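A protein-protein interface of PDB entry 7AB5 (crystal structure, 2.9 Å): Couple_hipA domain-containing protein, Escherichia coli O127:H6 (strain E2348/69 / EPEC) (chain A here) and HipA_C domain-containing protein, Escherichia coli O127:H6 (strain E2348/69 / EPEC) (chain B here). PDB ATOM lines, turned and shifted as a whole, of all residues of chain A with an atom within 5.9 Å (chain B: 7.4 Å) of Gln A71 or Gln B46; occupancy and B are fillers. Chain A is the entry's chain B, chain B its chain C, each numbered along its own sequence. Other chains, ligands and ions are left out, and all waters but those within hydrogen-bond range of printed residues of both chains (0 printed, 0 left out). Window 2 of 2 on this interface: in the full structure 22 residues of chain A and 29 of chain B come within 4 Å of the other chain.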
ATOM      1  N   TRP A  64       8.614  -0.527 -27.245  1.00  0.00           N
ATOM      2  CA  TRP A  64       9.125  -1.306 -26.121  1.00  0.00           C
ATOM      3  C   TRP A  64       8.222  -1.181 -24.900  1.00  0.00           C
ATOM      4  O   TRP A  64       8.063  -2.140 -24.134  1.00  0.00           O
ATOM      5  CB  TRP A  64      10.549  -0.853 -25.792  1.00  0.00           C
ATOM      6  CG  TRP A  64      11.321  -1.789 -24.908  1.00  0.00           C
ATOM      7  CD1 TRP A  64      12.124  -2.816 -25.307  1.00  0.00           C
ATOM      8  CD2 TRP A  64      11.383  -1.764 -23.476  1.00  0.00           C
ATOM      9  NE1 TRP A  64      12.673  -3.441 -24.214  1.00  0.00           N
ATOM     10  CE2 TRP A  64      12.233  -2.813 -23.077  1.00  0.00           C
ATOM     11  CE3 TRP A  64      10.798  -0.960 -22.494  1.00  0.00           C
ATOM     12  CZ2 TRP A  64      12.513  -3.079 -21.740  1.00  0.00           C
ATOM     13  CZ3 TRP A  64      11.077  -1.226 -21.167  1.00  0.00           C
ATOM     14  CH2 TRP A  64      11.926  -2.276 -20.802  1.00  0.00           C
ATOM     15  N   ARG A  66       4.898  -0.649 -24.950  1.00  0.00           N
ATOM     16  CA  ARG A  66       3.690  -1.439 -25.173  1.00  0.00           C
ATOM     17  C   ARG A  66       3.981  -2.931 -25.087  1.00  0.00           C
ATOM     18  O   ARG A  66       3.093  -3.716 -24.733  1.00  0.00           O
ATOM     19  CB  ARG A  66       3.064  -1.097 -26.529  1.00  0.00           C
ATOM     20  CG  ARG A  66       1.719  -1.781 -26.782  1.00  0.00           C
ATOM     21  CD  ARG A  66       0.897  -1.137 -27.903  1.00  0.00           C
ATOM     22  NE  ARG A  66       1.030   0.313 -27.984  1.00  0.00           N
ATOM     23  CZ  ARG A  66       0.024   1.143 -28.227  1.00  0.00           C
ATOM     24  NH1 ARG A  66      -1.211   0.702 -28.398  1.00  0.00           N
ATOM     25  NH2 ARG A  66       0.262   2.450 -28.290  1.00  0.00           N
ATOM     26  N   GLN A  67       5.214  -3.342 -25.392  1.00  0.00           N
ATOM     27  CA  GLN A  67       5.565  -4.756 -25.327  1.00  0.00           C
ATOM     28  C   GLN A  67       5.742  -5.224 -23.886  1.00  0.00           C
ATOM     29  O   GLN A  67       5.242  -6.288 -23.507  1.00  0.00           O
ATOM     30  CB  GLN A  67       6.836  -5.022 -26.134  1.00  0.00           C
ATOM     31  CG  GLN A  67       6.957  -6.451 -26.632  1.00  0.00           C
ATOM     32  CD  GLN A  67       8.305  -6.739 -27.255  1.00  0.00           C
ATOM     33  OE1 GLN A  67       8.784  -7.872 -27.224  1.00  0.00           O
ATOM     34  NE2 GLN A  67       8.925  -5.714 -27.828  1.00  0.00           N
ATOM     35  N   ARG A  68       6.457  -4.443 -23.068  1.00  0.00           N
ATOM     36  CA  ARG A  68       6.660  -4.828 -21.674  1.00  0.00           C
ATOM     37  C   ARG A  68       5.346  -4.865 -20.905  1.00  0.00           C
ATOM     38  O   ARG A  68       5.185  -5.685 -19.993  1.00  0.00           O
ATOM     39  CB  ARG A  68       7.643  -3.874 -20.992  1.00  0.00           C
ATOM     40  CG  ARG A  68       8.395  -4.510 -19.828  1.00  0.00           C
ATOM     41  CD  ARG A  68       9.128  -3.487 -18.961  1.00  0.00           C
ATOM     42  NE  ARG A  68       8.386  -2.244 -18.781  1.00  0.00           N
ATOM     43  CZ  ARG A  68       8.824  -1.213 -18.071  1.00  0.00           C
ATOM     44  NH1 ARG A  68       9.998  -1.243 -17.460  1.00  0.00           N
ATOM     45  NH2 ARG A  68       8.064  -0.126 -17.969  1.00  0.00           N
ATOM     46  N   TYR A  69       4.399  -3.996 -21.257  1.00  0.00           N
ATOM     47  CA  TYR A  69       3.115  -3.975 -20.568  1.00  0.00           C
ATOM     48  C   TYR A  69       2.208  -5.120 -21.001  1.00  0.00           C
ATOM     49  O   TYR A  69       1.434  -5.632 -20.185  1.00  0.00           O
ATOM     50  CB  TYR A  69       2.414  -2.636 -20.805  1.00  0.00           C
ATOM     51  CG  TYR A  69       0.912  -2.695 -20.635  1.00  0.00           C
ATOM     52  CD1 TYR A  69       0.341  -2.785 -19.374  1.00  0.00           C
ATOM     53  CD2 TYR A  69       0.066  -2.668 -21.738  1.00  0.00           C
ATOM     54  CE1 TYR A  69      -1.028  -2.846 -19.211  1.00  0.00           C
ATOM     55  CE2 TYR A  69      -1.305  -2.728 -21.585  1.00  0.00           C
ATOM     56  CZ  TYR A  69      -1.847  -2.816 -20.320  1.00  0.00           C
ATOM     57  OH  TYR A  69      -3.213  -2.875 -20.162  1.00  0.00           O
ATOM     58  N   SER A  70       2.293  -5.543 -22.263  1.00  0.00           N
ATOM     59  CA  SER A  70       1.365  -6.527 -22.808  1.00  0.00           C
ATOM     60  C   SER A  70       1.858  -7.964 -22.688  1.00  0.00           C
ATOM     61  O   SER A  70       1.064  -8.888 -22.892  1.00  0.00           O
ATOM     62  CB  SER A  70       1.068  -6.212 -24.278  1.00  0.00           C
ATOM     63  OG  SER A  70       1.963  -6.893 -25.138  1.00  0.00           O
ATOM     64  N   GLN A  71       3.137  -8.181 -22.374  1.00  0.00           N
ATOM     65  CA  GLN A  71       3.619  -9.537 -22.141  1.00  0.00           C
ATOM     66  C   GLN A  71       3.218 -10.063 -20.770  1.00  0.00           C
ATOM     67  O   GLN A  71       3.280 -11.277 -20.542  1.00  0.00           O
ATOM     68  CB  GLN A  71       5.142  -9.596 -22.287  1.00  0.00           C
ATOM     69  CG  GLN A  71       5.897  -8.776 -21.253  1.00  0.00           C
ATOM     70  CD  GLN A  71       7.360  -9.164 -21.153  1.00  0.00           C
ATOM     71  OE1 GLN A  71       7.932  -9.725 -22.088  1.00  0.00           O
ATOM     72  NE2 GLN A  71       7.975  -8.866 -20.013  1.00  0.00           N
ATOM     73  N   ILE A  72       2.804  -9.183 -19.864  1.00  0.00           N
ATOM     74  CA  ILE A  72       2.419  -9.583 -18.517  1.00  0.00           C
ATOM     75  C   ILE A  72       0.956  -9.290 -18.207  1.00  0.00           C
ATOM     76  O   ILE A  72       0.394  -9.919 -17.295  1.00  0.00           O
ATOM     77  CB  ILE A  72       3.335  -8.915 -17.467  1.00  0.00           C
ATOM     78  CG1 ILE A  72       3.187  -9.584 -16.097  1.00  0.00           C
ATOM     79  CG2 ILE A  72       3.064  -7.418 -17.385  1.00  0.00           C
ATOM     80  CD1 ILE A  72       4.420  -9.469 -15.227  1.00  0.00           C
ATOM     81  N   GLN A  73       0.305  -8.382 -18.930  1.00  0.00           N
ATOM     82  CA  GLN A  73      -1.103  -8.051 -18.721  1.00  0.00           C
ATOM     83  C   GLN A  73      -1.851  -8.322 -20.023  1.00  0.00           C
ATOM     84  O   GLN A  73      -1.733  -7.556 -20.986  1.00  0.00           O
ATOM     85  CB  GLN A  73      -1.265  -6.600 -18.277  1.00  0.00           C
ATOM     86  CG  GLN A  73      -2.126  -6.417 -17.035  1.00  0.00           C
ATOM     87  CD  GLN A  73      -3.581  -6.782 -17.267  1.00  0.00           C
ATOM     88  OE1 GLN A  73      -4.058  -6.802 -18.402  1.00  0.00           O
ATOM     89  NE2 GLN A  73      -4.296  -7.072 -16.186  1.00  0.00           N
ATOM     90  N   ARG B  41      22.223  -2.189 -15.911  1.00  0.00           N
ATOM     91  CA  ARG B  41      21.197  -2.194 -16.952  1.00  0.00           C
ATOM     92  C   ARG B  41      20.171  -3.293 -16.709  1.00  0.00           C
ATOM     93  O   ARG B  41      18.962  -3.033 -16.683  1.00  0.00           O
ATOM     94  CB  ARG B  41      21.840  -2.360 -18.328  1.00  0.00           C
ATOM     95  CG  ARG B  41      20.843  -2.757 -19.406  1.00  0.00           C
ATOM     96  CD  ARG B  41      21.269  -2.299 -20.787  1.00  0.00           C
ATOM     97  NE  ARG B  41      20.158  -2.360 -21.729  1.00  0.00           N
ATOM     98  CZ  ARG B  41      20.296  -2.455 -23.044  1.00  0.00           C
ATOM     99  NH1 ARG B  41      21.489  -2.507 -23.612  1.00  0.00           N
ATOM    100  NH2 ARG B  41      19.208  -2.502 -23.809  1.00  0.00           N
ATOM    101  N   THR B  42      20.636  -4.531 -16.527  1.00  0.00           N
ATOM    102  CA  THR B  42      19.737  -5.657 -16.301  1.00  0.00           C
ATOM    103  C   THR B  42      18.935  -5.520 -15.013  1.00  0.00           C
ATOM    104  O   THR B  42      18.020  -6.320 -14.782  1.00  0.00           O
ATOM    105  CB  THR B  42      20.537  -6.961 -16.278  1.00  0.00           C
ATOM    106  OG1 THR B  42      21.480  -6.927 -15.200  1.00  0.00           O
ATOM    107  CG2 THR B  42      21.289  -7.143 -17.587  1.00  0.00           C
ATOM    108  N   GLN B  43      19.255  -4.533 -14.173  1.00  0.00           N
ATOM    109  CA  GLN B  43      18.496  -4.309 -12.949  1.00  0.00           C
ATOM    110  C   GLN B  43      17.081  -3.833 -13.254  1.00  0.00           C
ATOM    111  O   GLN B  43      16.131  -4.204 -12.554  1.00  0.00           O
ATOM    112  CB  GLN B  43      19.221  -3.289 -12.073  1.00  0.00           C
ATOM    113  CG  GLN B  43      19.346  -3.666 -10.612  1.00  0.00           C
ATOM    114  CD  GLN B  43      19.968  -2.553  -9.788  1.00  0.00           C
ATOM    115  OE1 GLN B  43      21.173  -2.309  -9.864  1.00  0.00           O
ATOM    116  NE2 GLN B  43      19.147  -1.868  -9.000  1.00  0.00           N
ATOM    117  N   PHE B  44      16.920  -3.013 -14.293  1.00  0.00           N
ATOM    118  CA  PHE B  44      15.634  -2.388 -14.576  1.00  0.00           C
ATOM    119  C   PHE B  44      15.171  -2.673 -15.998  1.00  0.00           C
ATOM    120  O   PHE B  44      13.967  -2.688 -16.272  1.00  0.00           O
ATOM    121  CB  PHE B  44      15.721  -0.878 -14.343  1.00  0.00           C
ATOM    122  CG  PHE B  44      15.801  -0.492 -12.893  1.00  0.00           C
ATOM    123  CD1 PHE B  44      14.649  -0.282 -12.154  1.00  0.00           C
ATOM    124  CD2 PHE B  44      17.028  -0.346 -12.268  1.00  0.00           C
ATOM    125  CE1 PHE B  44      14.720   0.071 -10.819  1.00  0.00           C
ATOM    126  CE2 PHE B  44      17.106   0.006 -10.933  1.00  0.00           C
ATOM    127  CZ  PHE B  44      15.950   0.213 -10.208  1.00  0.00           C
ATOM    128  N   VAL B  45      16.114  -2.893 -16.910  1.00  0.00           N
ATOM    129  CA  VAL B  45      15.791  -3.146 -18.310  1.00  0.00           C
ATOM    130  C   VAL B  45      15.665  -4.654 -18.498  1.00  0.00           C
ATOM    131  O   VAL B  45      16.657  -5.386 -18.433  1.00  0.00           O
ATOM    132  CB  VAL B  45      16.844  -2.547 -19.251  1.00  0.00           C
ATOM    133  CG1 VAL B  45      16.750  -3.180 -20.635  1.00  0.00           C
ATOM    134  CG2 VAL B  45      16.673  -1.040 -19.340  1.00  0.00           C
ATOM    135  N   GLN B  46      14.439  -5.119 -18.715  1.00  0.00           N
ATOM    136  CA  GLN B  46      14.208  -6.516 -19.040  1.00  0.00           C
ATOM    137  C   GLN B  46      14.528  -6.763 -20.506  1.00  0.00           C
ATOM    138  O   GLN B  46      14.271  -5.915 -21.366  1.00  0.00           O
ATOM    139  CB  GLN B  46      12.761  -6.903 -18.733  1.00  0.00           C
ATOM    140  CG  GLN B  46      12.114  -6.042 -17.658  1.00  0.00           C
ATOM    141  CD  GLN B  46      10.732  -6.527 -17.270  1.00  0.00           C
ATOM    142  OE1 GLN B  46      10.071  -7.229 -18.034  1.00  0.00           O
ATOM    143  NE2 GLN B  46      10.289  -6.155 -16.076  1.00  0.00           N
ATOM    144  N   GLU B  47      15.104  -7.927 -20.788  1.00  0.00           N
ATOM    145  CA  GLU B  47      15.546  -8.269 -22.136  1.00  0.00           C
ATOM    146  C   GLU B  47      14.339  -8.770 -22.920  1.00  0.00           C
ATOM    147  O   GLU B  47      13.987  -9.951 -22.860  1.00  0.00           O
ATOM    148  CB  GLU B  47      16.662  -9.306 -22.073  1.00  0.00           C
ATOM    149  CG  GLU B  47      17.170  -9.803 -23.414  1.00  0.00           C
ATOM    150  CD  GLU B  47      18.512 -10.500 -23.287  1.00  0.00           C
ATOM    151  OE1 GLU B  47      19.119 -10.830 -24.328  1.00  0.00           O
ATOM    152  OE2 GLU B  47      18.960 -10.716 -22.140  1.00  0.00           O
ATOM    153  N   LEU B  48      13.692  -7.862 -23.652  1.00  0.00           N
ATOM    154  CA  LEU B  48      12.461  -8.197 -24.356  1.00  0.00           C
ATOM    155  C   LEU B  48      12.778  -8.840 -25.705  1.00  0.00           C
ATOM    156  O   LEU B  48      13.749  -8.458 -26.363  1.00  0.00           O
ATOM    157  CB  LEU B  48      11.606  -6.948 -24.562  1.00  0.00           C
ATOM    158  CG  LEU B  48      10.939  -6.367 -23.311  1.00  0.00           C
ATOM    159  CD1 LEU B  48       9.798  -5.436 -23.689  1.00  0.00           C
ATOM    160  CD2 LEU B  48      10.447  -7.477 -22.391  1.00  0.00           C
ATOM    161  N   PRO B  49      11.980  -9.816 -26.134  1.00  0.00           N
ATOM    162  CA  PRO B  49      12.210 -10.430 -27.445  1.00  0.00           C
ATOM    163  C   PRO B  49      11.987  -9.432 -28.569  1.00  0.00           C
ATOM    164  O   PRO B  49      11.217  -8.478 -28.441  1.00  0.00           O
ATOM    165  CB  PRO B  49      11.174 -11.560 -27.496  1.00  0.00           C
ATOM    166  CG  PRO B  49      10.119 -11.153 -26.518  1.00  0.00           C
ATOM    167  CD  PRO B  49      10.849 -10.436 -25.423  1.00  0.00           C
ATOM    168  N   PRO B  62      14.315   0.796 -25.312  1.00  0.00           N
ATOM    169  CA  PRO B  62      13.731   0.885 -23.971  1.00  0.00           C
ATOM    170  C   PRO B  62      13.726   2.323 -23.472  1.00  0.00           C
ATOM    171  O   PRO B  62      14.469   3.184 -23.949  1.00  0.00           O
ATOM    172  CB  PRO B  62      14.654   0.005 -23.119  1.00  0.00           C
ATOM    173  CG  PRO B  62      15.358  -0.880 -24.108  1.00  0.00           C
ATOM    174  CD  PRO B  62      15.536  -0.026 -25.323  1.00  0.00           C
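The side-chain amide oxygen (OE1) of Gln A67 lies close to the backbone carbonyl oxygen (O) of Pro B49, 2.8 Å away. NE2 of Gln A71 is in hydrogen-bond range of OE1 of Gln B46 (3.3 Å).
O of Gln B46 touches CZ2 of Trp A64, 3.4 Å away. Trp A64 touches Leu B48. CA of Pro B62 touches CD2 of Trp A64 (3.6 Å). CB of Gln A67 touches CD1 of Leu B48 (3.9 Å). Arg A68 touches Gln B46. Leu B48 touches Arg A68. Leu B48 touches Gln A71 (CD2 to OE1, 3.4 Å).
Hydrophobic or aromatic side chains of chain B that line the printed part of chain A: Leu B48, Pro B49 and Pro B62. Of the 9 printed residues of chain A, 4 touch a printed residue of chain B. Hydrophobic or aromatic side chains of chain A within 4 Å of the printed part of chain B: Trp A64. Along chain A the printed residues that touch a printed residue of chain B span positions 64 to 71. Among the printed residues, 9 pairs touch across the chains. Among the printed residues, no Asp or Glu carboxylate lies within 4 Å of a Lys or Arg side-chain nitrogen of the other chain.
Printed residues of chain B within 4 Å of Gln A67: Leu B48 (3.9 Å) and Pro B49 (2.8 Å). Of the printed residues of chain B, Arg A68 touches Gln B46 (3.7 Å) and Leu B48 (3.5 Å). Of chain B, only Gln B46 and Leu B48 come within 4 Å of Gln A71. Gln B46 touches three residues of chain A. Of the printed residues of chain A, Leu B48 touches Trp A64 (3.5 Å), Gln A67 (3.9 Å), Arg A68 (3.5 Å) and Gln A71 (3.4 Å). Printed residues of chain A within 4 Å of Pro B49: Gln A67 (2.8 Å). The nearest residue of chain B that does not touch Gln A71 is Pro B49 (4.5 Å). The nearest printed residue of chain A that does not touch Gln B46 is Ile A72 (6.7 Å).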
